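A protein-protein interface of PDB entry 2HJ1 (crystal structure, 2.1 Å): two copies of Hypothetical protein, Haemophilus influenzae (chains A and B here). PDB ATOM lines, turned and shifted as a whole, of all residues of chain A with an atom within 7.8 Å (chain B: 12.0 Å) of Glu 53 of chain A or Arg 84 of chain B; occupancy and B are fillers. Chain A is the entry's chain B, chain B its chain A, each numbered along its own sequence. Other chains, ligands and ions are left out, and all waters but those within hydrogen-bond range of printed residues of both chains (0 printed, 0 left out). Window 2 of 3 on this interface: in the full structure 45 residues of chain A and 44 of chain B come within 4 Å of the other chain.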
ATOM      1  N   ALA A  18       9.347  15.319  22.936  1.00  0.00           N
ATOM      2  CA  ALA A  18       9.215  16.739  23.288  1.00  0.00           C
ATOM      3  C   ALA A  18       7.820  16.995  23.827  1.00  0.00           C
ATOM      4  O   ALA A  18       6.848  16.439  23.325  1.00  0.00           O
ATOM      5  CB  ALA A  18       9.449  17.652  22.045  1.00  0.00           C
ATOM      6  N   TYR A  19       7.741  17.861  24.815  1.00  0.00           N
ATOM      7  CA  TYR A  19       6.478  18.236  25.395  1.00  0.00           C
ATOM      8  C   TYR A  19       6.700  19.580  26.045  1.00  0.00           C
ATOM      9  O   TYR A  19       7.608  19.730  26.861  1.00  0.00           O
ATOM     10  CB  TYR A  19       6.048  17.206  26.459  1.00  0.00           C
ATOM     11  CG  TYR A  19       4.741  17.532  27.174  1.00  0.00           C
ATOM     12  CD1 TYR A  19       3.499  17.504  26.504  1.00  0.00           C
ATOM     13  CD2 TYR A  19       4.751  17.830  28.513  1.00  0.00           C
ATOM     14  CE1 TYR A  19       2.284  17.816  27.190  1.00  0.00           C
ATOM     15  CE2 TYR A  19       3.548  18.109  29.205  1.00  0.00           C
ATOM     16  CZ  TYR A  19       2.350  18.106  28.543  1.00  0.00           C
ATOM     17  OH  TYR A  19       1.224  18.374  29.289  1.00  0.00           O
ATOM     18  N   ALA A  20       5.850  20.551  25.767  1.00  0.00           N
ATOM     19  CA  ALA A  20       6.201  21.918  26.198  1.00  0.00           C
ATOM     20  C   ALA A  20       5.466  22.336  27.447  1.00  0.00           C
ATOM     21  O   ALA A  20       4.402  22.911  27.384  1.00  0.00           O
ATOM     22  CB  ALA A  20       5.975  22.913  25.114  1.00  0.00           C
ATOM     23  N   PHE A  21       6.058  22.026  28.588  1.00  0.00           N
ATOM     24  CA  PHE A  21       5.526  22.426  29.855  1.00  0.00           C
ATOM     25  C   PHE A  21       5.937  23.885  29.938  1.00  0.00           C
ATOM     26  O   PHE A  21       7.148  24.187  30.077  1.00  0.00           O
ATOM     27  CB  PHE A  21       6.154  21.579  30.950  1.00  0.00           C
ATOM     28  CG  PHE A  21       5.638  21.862  32.330  1.00  0.00           C
ATOM     29  CD1 PHE A  21       6.504  22.310  33.325  1.00  0.00           C
ATOM     30  CD2 PHE A  21       4.284  21.616  32.660  1.00  0.00           C
ATOM     31  CE1 PHE A  21       6.037  22.528  34.624  1.00  0.00           C
ATOM     32  CE2 PHE A  21       3.819  21.834  33.958  1.00  0.00           C
ATOM     33  CZ  PHE A  21       4.704  22.300  34.932  1.00  0.00           C
ATOM     34  N   PRO A  22       4.927  24.796  29.812  1.00  0.00           N
ATOM     35  CA  PRO A  22       5.250  26.211  29.559  1.00  0.00           C
ATOM     36  C   PRO A  22       6.009  26.762  30.791  1.00  0.00           C
ATOM     37  O   PRO A  22       5.645  26.511  31.968  1.00  0.00           O
ATOM     38  CB  PRO A  22       3.881  26.869  29.288  1.00  0.00           C
ATOM     39  CG  PRO A  22       2.877  25.972  30.050  1.00  0.00           C
ATOM     40  CD  PRO A  22       3.469  24.556  29.962  1.00  0.00           C
ATOM     41  N   ILE A  47       7.845  10.122  31.019  1.00  0.00           N
ATOM     42  CA  ILE A  47       7.195  11.436  30.808  1.00  0.00           C
ATOM     43  C   ILE A  47       5.766  11.443  31.402  1.00  0.00           C
ATOM     44  O   ILE A  47       5.311  12.466  31.926  1.00  0.00           O
ATOM     45  CB  ILE A  47       7.189  11.874  29.319  1.00  0.00           C
ATOM     46  CG1 ILE A  47       6.802  13.356  29.186  1.00  0.00           C
ATOM     47  CG2 ILE A  47       6.218  11.031  28.433  1.00  0.00           C
ATOM     48  CD1 ILE A  47       6.687  13.810  27.787  1.00  0.00           C
ATOM     49  N   LEU A  48       5.078  10.296  31.352  1.00  0.00           N
ATOM     50  CA  LEU A  48       3.709  10.251  31.863  1.00  0.00           C
ATOM     51  C   LEU A  48       3.665  10.341  33.376  1.00  0.00           C
ATOM     52  O   LEU A  48       2.692  10.826  33.896  1.00  0.00           O
ATOM     53  CB  LEU A  48       2.932   9.027  31.375  1.00  0.00           C
ATOM     54  CG  LEU A  48       2.921   8.820  29.876  1.00  0.00           C
ATOM     55  CD1 LEU A  48       2.259   7.468  29.571  1.00  0.00           C
ATOM     56  CD2 LEU A  48       2.257   9.964  29.137  1.00  0.00           C
ATOM     57  N   SER A  49       4.717   9.900  34.068  1.00  0.00           N
ATOM     58  CA  SER A  49       4.831  10.142  35.533  1.00  0.00           C
ATOM     59  C   SER A  49       5.138  11.602  35.887  1.00  0.00           C
ATOM     60  O   SER A  49       4.580  12.149  36.848  1.00  0.00           O
ATOM     61  CB  SER A  49       5.877   9.212  36.162  1.00  0.00           C
ATOM     62  OG  SER A  49       5.562   7.865  35.802  1.00  0.00           O
ATOM     63  N   GLN A  50       6.006  12.246  35.107  1.00  0.00           N
ATOM     64  CA  GLN A  50       6.337  13.631  35.350  1.00  0.00           C
ATOM     65  C   GLN A  50       5.141  14.541  35.019  1.00  0.00           C
ATOM     66  O   GLN A  50       4.917  15.544  35.691  1.00  0.00           O
ATOM     67  CB  GLN A  50       7.565  14.026  34.519  1.00  0.00           C
ATOM     68  CG  GLN A  50       8.057  15.460  34.799  1.00  0.00           C
ATOM     69  CD  GLN A  50       9.329  15.780  34.057  1.00  0.00           C
ATOM     70  OE1 GLN A  50       9.901  14.916  33.378  1.00  0.00           O
ATOM     71  NE2 GLN A  50       9.776  17.025  34.159  1.00  0.00           N
ATOM     72  N   PHE A  51       4.400  14.231  33.965  1.00  0.00           N
ATOM     73  CA  PHE A  51       3.247  15.062  33.607  1.00  0.00           C
ATOM     74  C   PHE A  51       1.987  14.215  33.543  1.00  0.00           C
ATOM     75  O   PHE A  51       1.598  13.790  32.469  1.00  0.00           O
ATOM     76  CB  PHE A  51       3.485  15.727  32.262  1.00  0.00           C
ATOM     77  CG  PHE A  51       4.753  16.547  32.203  1.00  0.00           C
ATOM     78  CD1 PHE A  51       4.788  17.832  32.724  1.00  0.00           C
ATOM     79  CD2 PHE A  51       5.897  16.037  31.621  1.00  0.00           C
ATOM     80  CE1 PHE A  51       5.971  18.594  32.671  1.00  0.00           C
ATOM     81  CE2 PHE A  51       7.044  16.788  31.553  1.00  0.00           C
ATOM     82  CZ  PHE A  51       7.079  18.065  32.069  1.00  0.00           C
ATOM     83  N   PRO A  52       1.341  13.973  34.703  1.00  0.00           N
ATOM     84  CA  PRO A  52       0.184  13.079  34.692  1.00  0.00           C
ATOM     85  C   PRO A  52      -1.059  13.649  33.973  1.00  0.00           C
ATOM     86  O   PRO A  52      -2.010  12.894  33.698  1.00  0.00           O
ATOM     87  CB  PRO A  52      -0.059  12.799  36.170  1.00  0.00           C
ATOM     88  CG  PRO A  52       0.432  13.999  36.880  1.00  0.00           C
ATOM     89  CD  PRO A  52       1.608  14.524  36.054  1.00  0.00           C
ATOM     90  N   GLU A  53      -1.032  14.941  33.621  1.00  0.00           N
ATOM     91  CA  GLU A  53      -2.059  15.521  32.764  1.00  0.00           C
ATOM     92  C   GLU A  53      -2.009  15.052  31.304  1.00  0.00           C
ATOM     93  O   GLU A  53      -2.964  15.247  30.591  1.00  0.00           O
ATOM     94  CB  GLU A  53      -1.989  17.046  32.781  1.00  0.00           C
ATOM     95  CG  GLU A  53      -0.636  17.559  32.195  1.00  0.00           C
ATOM     96  CD  GLU A  53       0.424  17.865  33.269  1.00  0.00           C
ATOM     97  OE1 GLU A  53       0.968  18.984  33.227  1.00  0.00           O
ATOM     98  OE2 GLU A  53       0.704  17.050  34.161  1.00  0.00           O
ATOM     99  N   ILE A  54      -0.932  14.417  30.853  1.00  0.00           N
ATOM    100  CA  ILE A  54      -0.897  13.904  29.470  1.00  0.00           C
ATOM    101  C   ILE A  54      -1.868  12.697  29.366  1.00  0.00           C
ATOM    102  O   ILE A  54      -1.790  11.776  30.180  1.00  0.00           O
ATOM    103  CB  ILE A  54       0.514  13.456  29.038  1.00  0.00           C
ATOM    104  CG1 ILE A  54       1.476  14.665  28.897  1.00  0.00           C
ATOM    105  CG2 ILE A  54       0.478  12.648  27.709  1.00  0.00           C
ATOM    106  CD1 ILE A  54       2.964  14.212  28.666  1.00  0.00           C
ATOM    107  N   ASP A  55      -2.766  12.719  28.379  1.00  0.00           N
ATOM    108  CA  ASP A  55      -3.707  11.584  28.131  1.00  0.00           C
ATOM    109  C   ASP A  55      -3.430  11.105  26.733  1.00  0.00           C
ATOM    110  O   ASP A  55      -3.819  11.764  25.761  1.00  0.00           O
ATOM    111  CB  ASP A  55      -5.145  12.083  28.266  1.00  0.00           C
ATOM    112  CG  ASP A  55      -6.207  10.985  28.081  1.00  0.00           C
ATOM    113  OD1 ASP A  55      -5.904   9.891  27.562  1.00  0.00           O
ATOM    114  OD2 ASP A  55      -7.374  11.238  28.462  1.00  0.00           O
ATOM    115  N   LEU A  56      -2.745   9.967  26.619  1.00  0.00           N
ATOM    116  CA  LEU A  56      -2.433   9.387  25.305  1.00  0.00           C
ATOM    117  C   LEU A  56      -3.643   8.966  24.479  1.00  0.00           C
ATOM    118  O   LEU A  56      -3.523   8.803  23.263  1.00  0.00           O
ATOM    119  CB  LEU A  56      -1.486   8.174  25.432  1.00  0.00           C
ATOM    120  CG  LEU A  56      -0.072   8.488  25.939  1.00  0.00           C
ATOM    121  CD1 LEU A  56       0.764   7.235  25.897  1.00  0.00           C
ATOM    122  CD2 LEU A  56       0.610   9.646  25.093  1.00  0.00           C
ATOM    123  N   THR A  58      -6.247  10.712  23.847  1.00  0.00           N
ATOM    124  CA  THR A  58      -6.717  11.876  23.116  1.00  0.00           C
ATOM    125  C   THR A  58      -5.691  13.001  22.787  1.00  0.00           C
ATOM    126  O   THR A  58      -5.979  13.820  21.900  1.00  0.00           O
ATOM    127  CB  THR A  58      -7.864  12.582  23.843  1.00  0.00           C
ATOM    128  OG1 THR A  58      -7.365  13.172  25.040  1.00  0.00           O
ATOM    129  CG2 THR A  58      -9.051  11.599  24.171  1.00  0.00           C
ATOM    130  N   ASN A  59      -4.564  13.089  23.505  1.00  0.00           N
ATOM    131  CA  ASN A  59      -3.566  14.157  23.213  1.00  0.00           C
ATOM    132  C   ASN A  59      -3.136  14.153  21.748  1.00  0.00           C
ATOM    133  O   ASN A  59      -2.988  13.108  21.109  1.00  0.00           O
ATOM    134  CB  ASN A  59      -2.336  14.100  24.133  1.00  0.00           C
ATOM    135  CG  ASN A  59      -2.508  14.903  25.413  1.00  0.00           C
ATOM    136  OD1 ASN A  59      -1.582  15.598  25.840  1.00  0.00           O
ATOM    137  ND2 ASN A  59      -3.706  14.870  26.006  1.00  0.00           N
ATOM    138  N   LYS A  60      -2.991  15.341  21.196  1.00  0.00           N
ATOM    139  CA  LYS A  60      -2.470  15.446  19.847  1.00  0.00           C
ATOM    140  C   LYS A  60      -0.926  15.285  19.811  1.00  0.00           C
ATOM    141  O   LYS A  60      -0.210  15.788  20.680  1.00  0.00           O
ATOM    142  CB  LYS A  60      -3.011  16.714  19.182  1.00  0.00           C
ATOM    143  CG  LYS A  60      -4.439  16.401  18.581  1.00  0.00           C
ATOM    144  CD  LYS A  60      -5.490  17.484  18.859  1.00  0.00           C
ATOM    145  CE  LYS A  60      -6.967  16.909  18.850  1.00  0.00           C
ATOM    146  NZ  LYS A  60      -7.323  16.096  17.626  1.00  0.00           N
ATOM    147  N   PHE B  64       7.520  17.119   8.943  1.00  0.00           N
ATOM    148  CA  PHE B  64       6.631  17.082  10.090  1.00  0.00           C
ATOM    149  C   PHE B  64       5.305  16.416   9.709  1.00  0.00           C
ATOM    150  O   PHE B  64       4.659  16.824   8.731  1.00  0.00           O
ATOM    151  CB  PHE B  64       6.386  18.513  10.641  1.00  0.00           C
ATOM    152  CG  PHE B  64       5.372  18.529  11.760  1.00  0.00           C
ATOM    153  CD1 PHE B  64       5.716  18.042  13.022  1.00  0.00           C
ATOM    154  CD2 PHE B  64       4.061  18.945  11.529  1.00  0.00           C
ATOM    155  CE1 PHE B  64       4.777  18.003  14.052  1.00  0.00           C
ATOM    156  CE2 PHE B  64       3.119  18.921  12.566  1.00  0.00           C
ATOM    157  CZ  PHE B  64       3.486  18.436  13.823  1.00  0.00           C
ATOM    158  N   ARG B  66       1.436  15.014  11.212  1.00  0.00           N
ATOM    159  CA  ARG B  66       0.401  15.026  12.254  1.00  0.00           C
ATOM    160  C   ARG B  66      -0.968  14.910  11.592  1.00  0.00           C
ATOM    161  O   ARG B  66      -1.210  15.601  10.598  1.00  0.00           O
ATOM    162  CB  ARG B  66       0.454  16.326  13.075  1.00  0.00           C
ATOM    163  CG  ARG B  66      -0.523  16.343  14.261  1.00  0.00           C
ATOM    164  CD  ARG B  66      -0.740  17.755  14.759  1.00  0.00           C
ATOM    165  NE  ARG B  66      -2.104  17.946  15.259  1.00  0.00           N
ATOM    166  CZ  ARG B  66      -2.516  19.022  15.924  1.00  0.00           C
ATOM    167  NH1 ARG B  66      -3.768  19.110  16.338  1.00  0.00           N
ATOM    168  NH2 ARG B  66      -1.667  20.003  16.184  1.00  0.00           N
ATOM    169  N   ILE B  80       9.196  12.693  18.624  1.00  0.00           N
ATOM    170  CA  ILE B  80       7.780  12.657  19.018  1.00  0.00           C
ATOM    171  C   ILE B  80       7.408  13.952  19.695  1.00  0.00           C
ATOM    172  O   ILE B  80       8.006  14.294  20.699  1.00  0.00           O
ATOM    173  CB  ILE B  80       7.497  11.520  19.989  1.00  0.00           C
ATOM    174  CG1 ILE B  80       7.820  10.167  19.358  1.00  0.00           C
ATOM    175  CG2 ILE B  80       5.947  11.549  20.427  1.00  0.00           C
ATOM    176  CD1 ILE B  80       7.999   9.059  20.430  1.00  0.00           C
ATOM    177  N   GLU B  81       6.441  14.705  19.154  1.00  0.00           N
ATOM    178  CA  GLU B  81       6.028  15.915  19.827  1.00  0.00           C
ATOM    179  C   GLU B  81       4.619  15.688  20.405  1.00  0.00           C
ATOM    180  O   GLU B  81       3.701  15.477  19.640  1.00  0.00           O
ATOM    181  CB  GLU B  81       5.984  17.113  18.847  1.00  0.00           C
ATOM    182  CG  GLU B  81       7.308  17.221  18.054  1.00  0.00           C
ATOM    183  CD  GLU B  81       7.468  18.523  17.305  1.00  0.00           C
ATOM    184  OE1 GLU B  81       6.462  19.282  17.128  1.00  0.00           O
ATOM    185  OE2 GLU B  81       8.604  18.732  16.820  1.00  0.00           O
ATOM    186  N   ILE B  82       4.478  15.788  21.729  1.00  0.00           N
ATOM    187  CA  ILE B  82       3.189  15.669  22.415  1.00  0.00           C
ATOM    188  C   ILE B  82       2.706  17.099  22.697  1.00  0.00           C
ATOM    189  O   ILE B  82       3.424  17.878  23.280  1.00  0.00           O
ATOM    190  CB  ILE B  82       3.334  14.848  23.734  1.00  0.00           C
ATOM    191  CG1 ILE B  82       3.913  13.456  23.442  1.00  0.00           C
ATOM    192  CG2 ILE B  82       1.982  14.698  24.425  1.00  0.00           C
ATOM    193  CD1 ILE B  82       4.521  12.789  24.662  1.00  0.00           C
ATOM    194  N   TYR B  83       1.508  17.464  22.232  1.00  0.00           N
ATOM    195  CA  TYR B  83       1.031  18.844  22.409  1.00  0.00           C
ATOM    196  C   TYR B  83       0.125  18.989  23.636  1.00  0.00           C
ATOM    197  O   TYR B  83      -0.602  18.072  23.966  1.00  0.00           O
ATOM    198  CB  TYR B  83       0.290  19.318  21.150  1.00  0.00           C
ATOM    199  CG  TYR B  83       1.235  19.303  19.997  1.00  0.00           C
ATOM    200  CD1 TYR B  83       1.131  18.349  19.018  1.00  0.00           C
ATOM    201  CD2 TYR B  83       2.317  20.189  19.958  1.00  0.00           C
ATOM    202  CE1 TYR B  83       2.050  18.276  18.016  1.00  0.00           C
ATOM    203  CE2 TYR B  83       3.249  20.123  18.943  1.00  0.00           C
ATOM    204  CZ  TYR B  83       3.099  19.152  18.003  1.00  0.00           C
ATOM    205  OH  TYR B  83       3.974  19.114  17.008  1.00  0.00           O
ATOM    206  N   ARG B  84       0.168  20.149  24.287  1.00  0.00           N
ATOM    207  CA  ARG B  84      -0.880  20.490  25.277  1.00  0.00           C
ATOM    208  C   ARG B  84      -2.168  20.948  24.553  1.00  0.00           C
ATOM    209  O   ARG B  84      -2.099  21.789  23.651  1.00  0.00           O
ATOM    210  CB  ARG B  84      -0.355  21.534  26.286  1.00  0.00           C
ATOM    211  CG  ARG B  84       0.399  20.898  27.438  1.00  0.00           C
ATOM    212  CD  ARG B  84       1.400  21.802  28.110  1.00  0.00           C
ATOM    213  NE  ARG B  84       0.808  22.705  29.107  1.00  0.00           N
ATOM    214  CZ  ARG B  84       0.621  22.444  30.411  1.00  0.00           C
ATOM    215  NH1 ARG B  84       0.087  23.387  31.161  1.00  0.00           N
ATOM    216  NH2 ARG B  84       0.948  21.280  30.978  1.00  0.00           N
ATOM    217  N   PRO B  85      -3.340  20.357  24.903  1.00  0.00           N
ATOM    218  CA  PRO B  85      -4.639  20.796  24.312  1.00  0.00           C
ATOM    219  C   PRO B  85      -4.859  22.322  24.382  1.00  0.00           C
ATOM    220  O   PRO B  85      -4.531  22.948  25.394  1.00  0.00           O
ATOM    221  CB  PRO B  85      -5.691  20.074  25.172  1.00  0.00           C
ATOM    222  CG  PRO B  85      -4.982  18.843  25.661  1.00  0.00           C
ATOM    223  CD  PRO B  85      -3.521  19.245  25.863  1.00  0.00           C
ATOM    224  N   LEU B  86      -5.400  22.888  23.306  1.00  0.00           N
ATOM    225  CA  LEU B  86      -5.613  24.341  23.163  1.00  0.00           C
ATOM    226  C   LEU B  86      -6.737  24.878  24.070  1.00  0.00           C
ATOM    227  O   LEU B  86      -7.643  24.127  24.461  1.00  0.00           O
ATOM    228  CB  LEU B  86      -5.939  24.675  21.699  1.00  0.00           C
ATOM    229  CG  LEU B  86      -4.999  24.159  20.602  1.00  0.00           C
ATOM    230  CD1 LEU B  86      -5.775  23.923  19.300  1.00  0.00           C
ATOM    231  CD2 LEU B  86      -3.792  25.101  20.394  1.00  0.00           C
ATOM    232  N   LEU B  87      -6.710  26.176  24.386  1.00  0.00           N
ATOM    233  CA  LEU B  87      -5.740  27.136  23.837  1.00  0.00           C
ATOM    234  C   LEU B  87      -4.680  27.525  24.869  1.00  0.00           C
ATOM    235  O   LEU B  87      -4.617  28.676  25.316  1.00  0.00           O
ATOM    236  CB  LEU B  87      -6.464  28.381  23.268  1.00  0.00           C
ATOM    237  CG  LEU B  87      -6.999  28.306  21.827  1.00  0.00           C
ATOM    238  CD1 LEU B  87      -8.439  27.760  21.753  1.00  0.00           C
ATOM    239  CD2 LEU B  87      -6.904  29.682  21.136  1.00  0.00           C
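The backbone carbonyl oxygen (O) of Ile 80 of chain B lies within hydrogen-bond range of the backbone NH (N) of Ala 18 of chain A, 2.8 Å away.
The backbone NH (N) of Ile 82 of chain B is in hydrogen-bond range of the backbone carbonyl oxygen (O) of Ala 18 of chain A, 2.9 Å away.
The backbone carbonyl oxygen of Tyr 83 of chain B sits close to the side-chain amide oxygen of Asn 59 of chain A (3.3 Å).
The backbone carbonyl oxygen of Lys 60 of chain A lies within hydrogen-bond range of the backbone NH of Tyr 83 of chain B, at 2.9 Å.
The guanidinium group (NH2) of Arg 84 of chain B sits close to the side-chain hydroxyl (OH) of Tyr 19 of chain A.
NH2 of Arg 84 of chain B is in salt-bridge range of OE1 of Glu 53 of chain A (3.2 Å).
The side-chain carboxylate (OE1) of Glu 81 of chain B lies within hydrogen-bond range of the side-chain hydroxyl (OH) of Tyr 83 of chain B, 2.5 Å away.
O of Asp 55 of chain A lies within hydrogen-bond range of ND2 of Asn 59 of chain A.
O of Ala 18 of chain A touches CA of Glu 81 of chain B, at 3.6 Å.
CD1 of Tyr 19 of chain A touches O of Ile 82 of chain B, at 3.2 Å.
Ala 20 of chain A touches Arg 84 of chain B.
Arg 84 of chain B touches Phe 21 of chain A.
Arg 84 of chain B touches Pro 22 of chain A (NE to CD, 3.4 Å).
Ile 47 of chain A touches Ile 82 of chain B.
CG2 of Ile 82 of chain B touches OD1 of Asn 59 of chain A, at 3.9 Å.
Lys 60 of chain A touches Arg 66 of chain B.
Lys 60 of chain A touches Ile 82 of chain B (O to C, 3.8 Å).
Ala 20 of chain A touches just one residue of chain B: Arg 84 (3.3 Å).
Phe 21 of chain A touches one residue of chain B.
Pro 22 of chain A touches just one residue of chain B: Arg 84 (3.4 Å).
Printed residues of chain B within 4 Å of Ile 47 of chain A: Ile 82.
No residue of chain B comes within 4 Å of Pro 52 of chain A.
Of the printed residues of chain B, Glu 53 of chain A touches Arg 84 (3.2 Å).
No residue of chain B comes within 4 Å of Asp 55 of chain A.
Printed residues of chain B within 4 Å of Lys 60 of chain A: Arg 66, Ile 82 and Tyr 83.
Of the printed residues of chain A, Tyr 83 of chain B touches Asn 59 (3.3 Å) and Lys 60 (2.9 Å).
Arg 84 of chain B touches five residues of chain A.
No residue of chain A comes within 4 Å of Pro 85 of chain B.
Leu 86 of chain B touches none of the printed residues of chain A.
Leu 87 of chain B touches none of the printed residues of chain A.
The nearest residue of chain A that does not touch Arg 84 of chain B is Asn 59 of chain A (5.0 Å).
Hydrophobic or aromatic side chains of chain A that line the printed part of chain B: Ala 18, Tyr 19, Phe 21, Pro 22 and Ile 47.
Hydrophobic or aromatic side chains of chain B within 4 Å of the printed part of chain A: Ile 82 and Tyr 83.
Among the printed residues, Asp or Glu carboxylates within 4 Å of a Lys or Arg side-chain nitrogen of the other chain: Glu 53 of chain A with Arg 84 of chain B (3.2 Å).
No position is printed for both chains.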
